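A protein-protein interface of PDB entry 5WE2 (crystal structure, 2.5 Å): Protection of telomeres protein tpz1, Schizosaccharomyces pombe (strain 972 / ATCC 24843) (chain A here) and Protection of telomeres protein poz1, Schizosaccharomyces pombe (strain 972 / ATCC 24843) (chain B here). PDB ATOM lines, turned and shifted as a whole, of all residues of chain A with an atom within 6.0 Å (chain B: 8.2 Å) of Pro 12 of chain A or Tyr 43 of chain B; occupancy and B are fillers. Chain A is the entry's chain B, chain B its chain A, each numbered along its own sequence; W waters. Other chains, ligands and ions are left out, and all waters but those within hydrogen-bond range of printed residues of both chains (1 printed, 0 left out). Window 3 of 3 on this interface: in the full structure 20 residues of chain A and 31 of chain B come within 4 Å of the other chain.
Hydrophobic or aromatic side chains of chain B that line the printed part of chain A: Tyr 43.
Of the 8 printed residues of chain A, 6 touch a printed residue of chain B.
Printed residues of chain A that touch a printed residue of chain B: Gly 10, Pro 12, His 13, Gly 14, Phe 17 and Leu 20.
Hydrophobic or aromatic side chains of chain A within 4 Å of the printed part of chain B: Pro 12, His 13, Phe 17 and Leu 20.
Among the printed residues, 9 pairs touch across the chains.
Among the printed residues, no Asp or Glu carboxylate lies within 4 Å of a Lys or Arg side-chain nitrogen of the other chain.
Of the printed residues of chain B, Leu 20 of chain A touches Leu 38, Arg 39 and Tyr 43.
Printed residues of chain A within 4 Å of Leu 38 of chain B: Leu 20.
Tyr 40 of chain B touches none of the printed residues of chain A.
Of the printed residues of chain A, Gly 42 of chain B touches Phe 17 (3.5 Å).
The nearest residue of chain B that does not touch Pro 12 of chain A is Gly 42 of chain B (4.1 Å).
The nearest printed residue of chain A that does not touch Tyr 43 of chain B is Leu 11 of chain A (6.5 Å).
The nearest printed residue of chain A that does not touch Arg 39 of chain B is Phe 17 of chain A (6.9 Å).
The backbone carbonyl oxygen of His 13 of chain A lies close to the side-chain sulfur of Cys 48 of chain B (3.7 Å).
Water W1 lies within hydrogen-bond range of the backbone carbonyl oxygen of Gly 42 of chain B, the backbone carbonyl oxygen of His 13 of chain A and the side-chain sulfur of Cys 48 of chain B.
O of Leu 11 of chain A is in hydrogen-bond range of ND1 of His 13 of chain A (2.7 Å).
The backbone NH (N) of Lys 45 of chain B lies within hydrogen-bond range of the side-chain carboxylate (OE1) of Glu 3 of chain B, at 3.3 Å.
The side-chain sulfur of Cys 48 of chain B sits at hydrogen-bond distance from the backbone carbonyl oxygen of Ser 44 of chain B, at 3.7 Å.
SG of Cys 48 of chain B sits close to O of Lys 45 of chain B (3.5 Å).
Among the printed residues, pairs that only touch across the chains: Gly 10 of chain A with Lys 45 of chain B (3.97 Å), Pro 12 of chain A with Tyr 43 of chain B (3.9 Å), Gly 14 of chain A with Cys 48 of chain B (3.7 Å), Phe 17 of chain A with Gly 42 of chain B (3.5 Å), Phe 17 of chain A with Tyr 43 of chain B (3.99 Å), Leu 20 of chain A with Leu 38 of chain B (3.7 Å), Leu 20 of chain A with Arg 39 of chain B (3.7 Å) and Leu 20 of chain A with Tyr 43 of chain B (3.6 Å).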
ATOM      1  N   MET A   6      34.021  -2.510 -14.813  1.00  0.00           N
ATOM      2  CA  MET A   6      33.063  -2.783 -15.884  1.00  0.00           C
ATOM      3  C   MET A   6      32.565  -1.474 -16.488  1.00  0.00           C
ATOM      4  O   MET A   6      32.392  -1.364 -17.710  1.00  0.00           O
ATOM      5  CB  MET A   6      31.909  -3.620 -15.350  1.00  0.00           C
ATOM      6  CG  MET A   6      32.353  -4.989 -14.845  1.00  0.00           C
ATOM      7  SD  MET A   6      33.029  -5.953 -16.204  1.00  0.00           S
ATOM      8  CE  MET A   6      31.504  -6.495 -17.010  1.00  0.00           C
ATOM      9  N   GLY A  10      33.133   0.236 -20.270  1.00  0.00           N
ATOM     10  CA  GLY A  10      31.824   0.309 -20.911  1.00  0.00           C
ATOM     11  C   GLY A  10      31.137  -1.031 -21.199  1.00  0.00           C
ATOM     12  O   GLY A  10      30.393  -1.163 -22.175  1.00  0.00           O
ATOM     13  N   LEU A  11      31.390  -2.044 -20.383  1.00  0.00           N
ATOM     14  CA  LEU A  11      30.699  -3.319 -20.576  1.00  0.00           C
ATOM     15  C   LEU A  11      29.367  -3.329 -19.798  1.00  0.00           C
ATOM     16  O   LEU A  11      29.273  -2.731 -18.718  1.00  0.00           O
ATOM     17  CB  LEU A  11      31.584  -4.482 -20.138  1.00  0.00           C
ATOM     18  CG  LEU A  11      32.931  -4.663 -20.842  1.00  0.00           C
ATOM     19  CD1 LEU A  11      33.742  -5.649 -20.069  1.00  0.00           C
ATOM     20  CD2 LEU A  11      32.758  -5.138 -22.286  1.00  0.00           C
ATOM     21  N   PRO A  12      28.334  -3.985 -20.354  1.00  0.00           N
ATOM     22  CA  PRO A  12      27.065  -4.097 -19.600  1.00  0.00           C
ATOM     23  C   PRO A  12      27.241  -4.961 -18.365  1.00  0.00           C
ATOM     24  O   PRO A  12      27.837  -6.027 -18.419  1.00  0.00           O
ATOM     25  CB  PRO A  12      26.089  -4.761 -20.604  1.00  0.00           C
ATOM     26  CG  PRO A  12      26.988  -5.614 -21.503  1.00  0.00           C
ATOM     27  CD  PRO A  12      28.340  -4.825 -21.574  1.00  0.00           C
ATOM     28  N   HIS A  13      26.763  -4.471 -17.242  1.00  0.00           N
ATOM     29  CA  HIS A  13      26.775  -5.229 -16.000  1.00  0.00           C
ATOM     30  C   HIS A  13      25.629  -4.733 -15.112  1.00  0.00           C
ATOM     31  O   HIS A  13      24.967  -3.756 -15.459  1.00  0.00           O
ATOM     32  CB  HIS A  13      28.116  -5.081 -15.293  1.00  0.00           C
ATOM     33  CG  HIS A  13      28.526  -3.653 -15.064  1.00  0.00           C
ATOM     34  ND1 HIS A  13      28.808  -2.777 -16.094  1.00  0.00           N
ATOM     35  CD2 HIS A  13      28.755  -2.979 -13.911  1.00  0.00           C
ATOM     36  CE1 HIS A  13      29.176  -1.608 -15.581  1.00  0.00           C
ATOM     37  NE2 HIS A  13      29.165  -1.713 -14.266  1.00  0.00           N
ATOM     38  N   GLY A  14      25.391  -5.385 -13.973  1.00  0.00           N
ATOM     39  CA  GLY A  14      24.431  -4.840 -13.021  1.00  0.00           C
ATOM     40  C   GLY A  14      23.009  -5.366 -13.170  1.00  0.00           C
ATOM     41  O   GLY A  14      22.730  -6.193 -14.047  1.00  0.00           O
ATOM     42  N   PHE A  17      20.887  -5.134 -16.392  1.00  0.00           N
ATOM     43  CA  PHE A  17      21.428  -6.016 -17.409  1.00  0.00           C
ATOM     44  C   PHE A  17      21.109  -7.477 -17.100  1.00  0.00           C
ATOM     45  O   PHE A  17      20.683  -8.248 -17.988  1.00  0.00           O
ATOM     46  CB  PHE A  17      22.955  -5.789 -17.553  1.00  0.00           C
ATOM     47  CG  PHE A  17      23.621  -6.740 -18.507  1.00  0.00           C
ATOM     48  CD1 PHE A  17      23.305  -6.718 -19.859  1.00  0.00           C
ATOM     49  CD2 PHE A  17      24.548  -7.674 -18.043  1.00  0.00           C
ATOM     50  CE1 PHE A  17      23.918  -7.611 -20.751  1.00  0.00           C
ATOM     51  CE2 PHE A  17      25.167  -8.564 -18.923  1.00  0.00           C
ATOM     52  CZ  PHE A  17      24.855  -8.531 -20.284  1.00  0.00           C
ATOM     53  N   LEU A  20      17.497  -8.057 -17.909  1.00  0.00           N
ATOM     54  CA  LEU A  20      17.351  -8.204 -19.355  1.00  0.00           C
ATOM     55  C   LEU A  20      17.657  -9.626 -19.834  1.00  0.00           C
ATOM     56  O   LEU A  20      16.900 -10.239 -20.626  1.00  0.00           O
ATOM     57  CB  LEU A  20      18.266  -7.216 -20.065  1.00  0.00           C
ATOM     58  CG  LEU A  20      18.404  -7.389 -21.572  1.00  0.00           C
ATOM     59  CD1 LEU A  20      17.093  -6.961 -22.240  1.00  0.00           C
ATOM     60  CD2 LEU A  20      19.662  -6.627 -22.111  1.00  0.00           C
ATOM     61  N   GLU B   3      21.260  10.756 -19.822  1.00  0.00           N
ATOM     62  CA  GLU B   3      20.911   9.347 -19.970  1.00  0.00           C
ATOM     63  C   GLU B   3      20.159   8.890 -18.728  1.00  0.00           C
ATOM     64  O   GLU B   3      19.205   8.131 -18.837  1.00  0.00           O
ATOM     65  CB  GLU B   3      22.114   8.427 -20.237  1.00  0.00           C
ATOM     66  CG  GLU B   3      21.624   6.982 -20.515  1.00  0.00           C
ATOM     67  CD  GLU B   3      22.704   6.016 -20.995  1.00  0.00           C
ATOM     68  OE1 GLU B   3      23.797   5.995 -20.382  1.00  0.00           O
ATOM     69  OE2 GLU B   3      22.446   5.253 -21.975  1.00  0.00           O
ATOM     70  N   SER B   7      16.499   7.258 -18.762  1.00  0.00           N
ATOM     71  CA  SER B   7      16.309   5.955 -18.156  1.00  0.00           C
ATOM     72  C   SER B   7      15.160   5.949 -17.175  1.00  0.00           C
ATOM     73  O   SER B   7      14.337   5.025 -17.183  1.00  0.00           O
ATOM     74  CB  SER B   7      17.598   5.501 -17.471  1.00  0.00           C
ATOM     75  OG  SER B   7      18.516   5.040 -18.450  1.00  0.00           O
ATOM     76  N   ALA B  36      12.360  -3.429 -26.009  1.00  0.00           N
ATOM     77  CA  ALA B  36      13.178  -2.241 -26.259  1.00  0.00           C
ATOM     78  C   ALA B  36      13.522  -1.486 -24.962  1.00  0.00           C
ATOM     79  O   ALA B  36      14.682  -1.066 -24.773  1.00  0.00           O
ATOM     80  CB  ALA B  36      12.484  -1.316 -27.245  1.00  0.00           C
ATOM     81  N   CYS B  37      12.537  -1.340 -24.068  1.00  0.00           N
ATOM     82  CA  CYS B  37      12.758  -0.714 -22.751  1.00  0.00           C
ATOM     83  C   CYS B  37      13.755  -1.451 -21.885  1.00  0.00           C
ATOM     84  O   CYS B  37      14.664  -0.840 -21.282  1.00  0.00           O
ATOM     85  CB  CYS B  37      11.432  -0.602 -21.972  1.00  0.00           C
ATOM     86  SG  CYS B  37      10.297   0.620 -22.683  1.00  0.00           S
ATOM     87  N   LEU B  38      13.550  -2.762 -21.783  1.00  0.00           N
ATOM     88  CA  LEU B  38      14.387  -3.586 -20.929  1.00  0.00           C
ATOM     89  C   LEU B  38      15.806  -3.548 -21.469  1.00  0.00           C
ATOM     90  O   LEU B  38      16.744  -3.497 -20.699  1.00  0.00           O
ATOM     91  CB  LEU B  38      13.857  -5.035 -20.840  1.00  0.00           C
ATOM     92  CG  LEU B  38      12.563  -5.270 -20.046  1.00  0.00           C
ATOM     93  CD1 LEU B  38      12.000  -6.681 -20.299  1.00  0.00           C
ATOM     94  CD2 LEU B  38      12.754  -5.009 -18.542  1.00  0.00           C
ATOM     95  N   ARG B  39      15.961  -3.529 -22.794  1.00  0.00           N
ATOM     96  CA  ARG B  39      17.293  -3.454 -23.401  1.00  0.00           C
ATOM     97  C   ARG B  39      17.965  -2.119 -23.181  1.00  0.00           C
ATOM     98  O   ARG B  39      19.166  -2.054 -22.850  1.00  0.00           O
ATOM     99  CB  ARG B  39      17.247  -3.747 -24.896  1.00  0.00           C
ATOM    100  CG  ARG B  39      18.509  -4.449 -25.357  1.00  0.00           C
ATOM    101  CD  ARG B  39      18.695  -4.471 -26.878  1.00  0.00           C
ATOM    102  NE  ARG B  39      19.952  -5.145 -27.237  1.00  0.00           N
ATOM    103  CZ  ARG B  39      21.151  -4.561 -27.281  1.00  0.00           C
ATOM    104  NH1 ARG B  39      21.291  -3.273 -26.989  1.00  0.00           N
ATOM    105  NH2 ARG B  39      22.224  -5.272 -27.607  1.00  0.00           N
ATOM    106  N   TYR B  40      17.226  -1.038 -23.368  1.00  0.00           N
ATOM    107  CA  TYR B  40      17.835   0.263 -23.090  1.00  0.00           C
ATOM    108  C   TYR B  40      18.302   0.316 -21.634  1.00  0.00           C
ATOM    109  O   TYR B  40      19.425   0.693 -21.367  1.00  0.00           O
ATOM    110  CB  TYR B  40      16.851   1.391 -23.387  1.00  0.00           C
ATOM    111  CG  TYR B  40      17.479   2.745 -23.285  1.00  0.00           C
ATOM    112  CD1 TYR B  40      18.140   3.295 -24.366  1.00  0.00           C
ATOM    113  CD2 TYR B  40      17.425   3.480 -22.100  1.00  0.00           C
ATOM    114  CE1 TYR B  40      18.726   4.544 -24.282  1.00  0.00           C
ATOM    115  CE2 TYR B  40      18.000   4.736 -22.011  1.00  0.00           C
ATOM    116  CZ  TYR B  40      18.657   5.257 -23.114  1.00  0.00           C
ATOM    117  OH  TYR B  40      19.265   6.493 -23.054  1.00  0.00           O
ATOM    118  N   LEU B  41      17.472  -0.093 -20.672  1.00  0.00           N
ATOM    119  CA  LEU B  41      17.935  -0.019 -19.288  1.00  0.00           C
ATOM    120  C   LEU B  41      19.106  -0.963 -19.062  1.00  0.00           C
ATOM    121  O   LEU B  41      20.044  -0.669 -18.308  1.00  0.00           O
ATOM    122  CB  LEU B  41      16.806  -0.355 -18.318  1.00  0.00           C
ATOM    123  CG  LEU B  41      15.667   0.642 -18.397  1.00  0.00           C
ATOM    124  CD1 LEU B  41      14.501   0.069 -17.682  1.00  0.00           C
ATOM    125  CD2 LEU B  41      16.122   1.960 -17.794  1.00  0.00           C
ATOM    126  N   GLY B  42      19.024  -2.116 -19.707  1.00  0.00           N
ATOM    127  CA  GLY B  42      20.089  -3.098 -19.667  1.00  0.00           C
ATOM    128  C   GLY B  42      21.447  -2.614 -20.150  1.00  0.00           C
ATOM    129  O   GLY B  42      22.467  -3.091 -19.651  1.00  0.00           O
ATOM    130  N   TYR B  43      21.482  -1.685 -21.108  1.00  0.00           N
ATOM    131  CA  TYR B  43      22.783  -1.190 -21.599  1.00  0.00           C
ATOM    132  C   TYR B  43      23.088   0.233 -21.216  1.00  0.00           C
ATOM    133  O   TYR B  43      24.083   0.787 -21.662  1.00  0.00           O
ATOM    134  CB  TYR B  43      22.881  -1.309 -23.117  1.00  0.00           C
ATOM    135  CG  TYR B  43      23.106  -2.728 -23.534  1.00  0.00           C
ATOM    136  CD1 TYR B  43      22.049  -3.611 -23.535  1.00  0.00           C
ATOM    137  CD2 TYR B  43      24.378  -3.197 -23.925  1.00  0.00           C
ATOM    138  CE1 TYR B  43      22.198  -4.904 -23.903  1.00  0.00           C
ATOM    139  CE2 TYR B  43      24.547  -4.546 -24.290  1.00  0.00           C
ATOM    140  CZ  TYR B  43      23.424  -5.385 -24.267  1.00  0.00           C
ATOM    141  OH  TYR B  43      23.456  -6.708 -24.611  1.00  0.00           O
ATOM    142  N   SER B  44      22.243   0.816 -20.384  1.00  0.00           N
ATOM    143  CA  SER B  44      22.429   2.183 -19.936  1.00  0.00           C
ATOM    144  C   SER B  44      23.500   2.241 -18.850  1.00  0.00           C
ATOM    145  O   SER B  44      23.358   1.598 -17.807  1.00  0.00           O
ATOM    146  CB  SER B  44      21.105   2.754 -19.424  1.00  0.00           C
ATOM    147  OG  SER B  44      21.339   3.902 -18.633  1.00  0.00           O
ATOM    148  N   LYS B  45      24.565   3.003 -19.092  1.00  0.00           N
ATOM    149  CA  LYS B  45      25.689   3.070 -18.165  1.00  0.00           C
ATOM    150  C   LYS B  45      25.239   3.640 -16.824  1.00  0.00           C
ATOM    151  O   LYS B  45      25.635   3.155 -15.757  1.00  0.00           O
ATOM    152  CB  LYS B  45      26.833   3.926 -18.739  1.00  0.00           C
ATOM    153  CG  LYS B  45      27.156   3.700 -20.207  1.00  0.00           C
ATOM    154  CD  LYS B  45      28.272   2.678 -20.399  1.00  0.00           C
ATOM    155  CE  LYS B  45      28.739   2.623 -21.861  1.00  0.00           C
ATOM    156  NZ  LYS B  45      29.425   3.885 -22.317  1.00  0.00           N
ATOM    157  N   SER B  46      24.388   4.658 -16.879  1.00  0.00           N
ATOM    158  CA  SER B  46      23.936   5.326 -15.656  1.00  0.00           C
ATOM    159  C   SER B  46      23.118   4.404 -14.736  1.00  0.00           C
ATOM    160  O   SER B  46      23.103   4.600 -13.515  1.00  0.00           O
ATOM    161  CB  SER B  46      23.115   6.568 -16.008  1.00  0.00           C
ATOM    162  OG  SER B  46      22.182   6.280 -17.031  1.00  0.00           O
ATOM    163  N   MET B  47      22.473   3.384 -15.311  1.00  0.00           N
ATOM    164  CA  MET B  47      21.656   2.479 -14.512  1.00  0.00           C
ATOM    165  C   MET B  47      22.462   1.339 -13.927  1.00  0.00           C
ATOM    166  O   MET B  47      21.912   0.576 -13.122  1.00  0.00           O
ATOM    167  CB  MET B  47      20.477   1.906 -15.329  1.00  0.00           C
ATOM    168  CG  MET B  47      19.492   2.981 -15.798  1.00  0.00           C
ATOM    169  SD  MET B  47      18.918   4.045 -14.432  1.00  0.00           S
ATOM    170  CE  MET B  47      17.589   3.025 -13.806  1.00  0.00           C
ATOM    171  N   CYS B  48      23.747   1.226 -14.282  1.00  0.00           N
ATOM    172  CA  CYS B  48      24.521   0.045 -13.829  1.00  0.00           C
ATOM    173  C   CYS B  48      24.603  -0.201 -12.310  1.00  0.00           C
ATOM    174  O   CYS B  48      24.865  -1.327 -11.861  1.00  0.00           O
ATOM    175  CB  CYS B  48      25.959   0.117 -14.377  1.00  0.00           C
ATOM    176  SG  CYS B  48      26.012  -0.278 -16.116  1.00  0.00           S
HETATM  177  O   HOH W   1      24.755  -2.227 -18.044  1.00  0.00           O
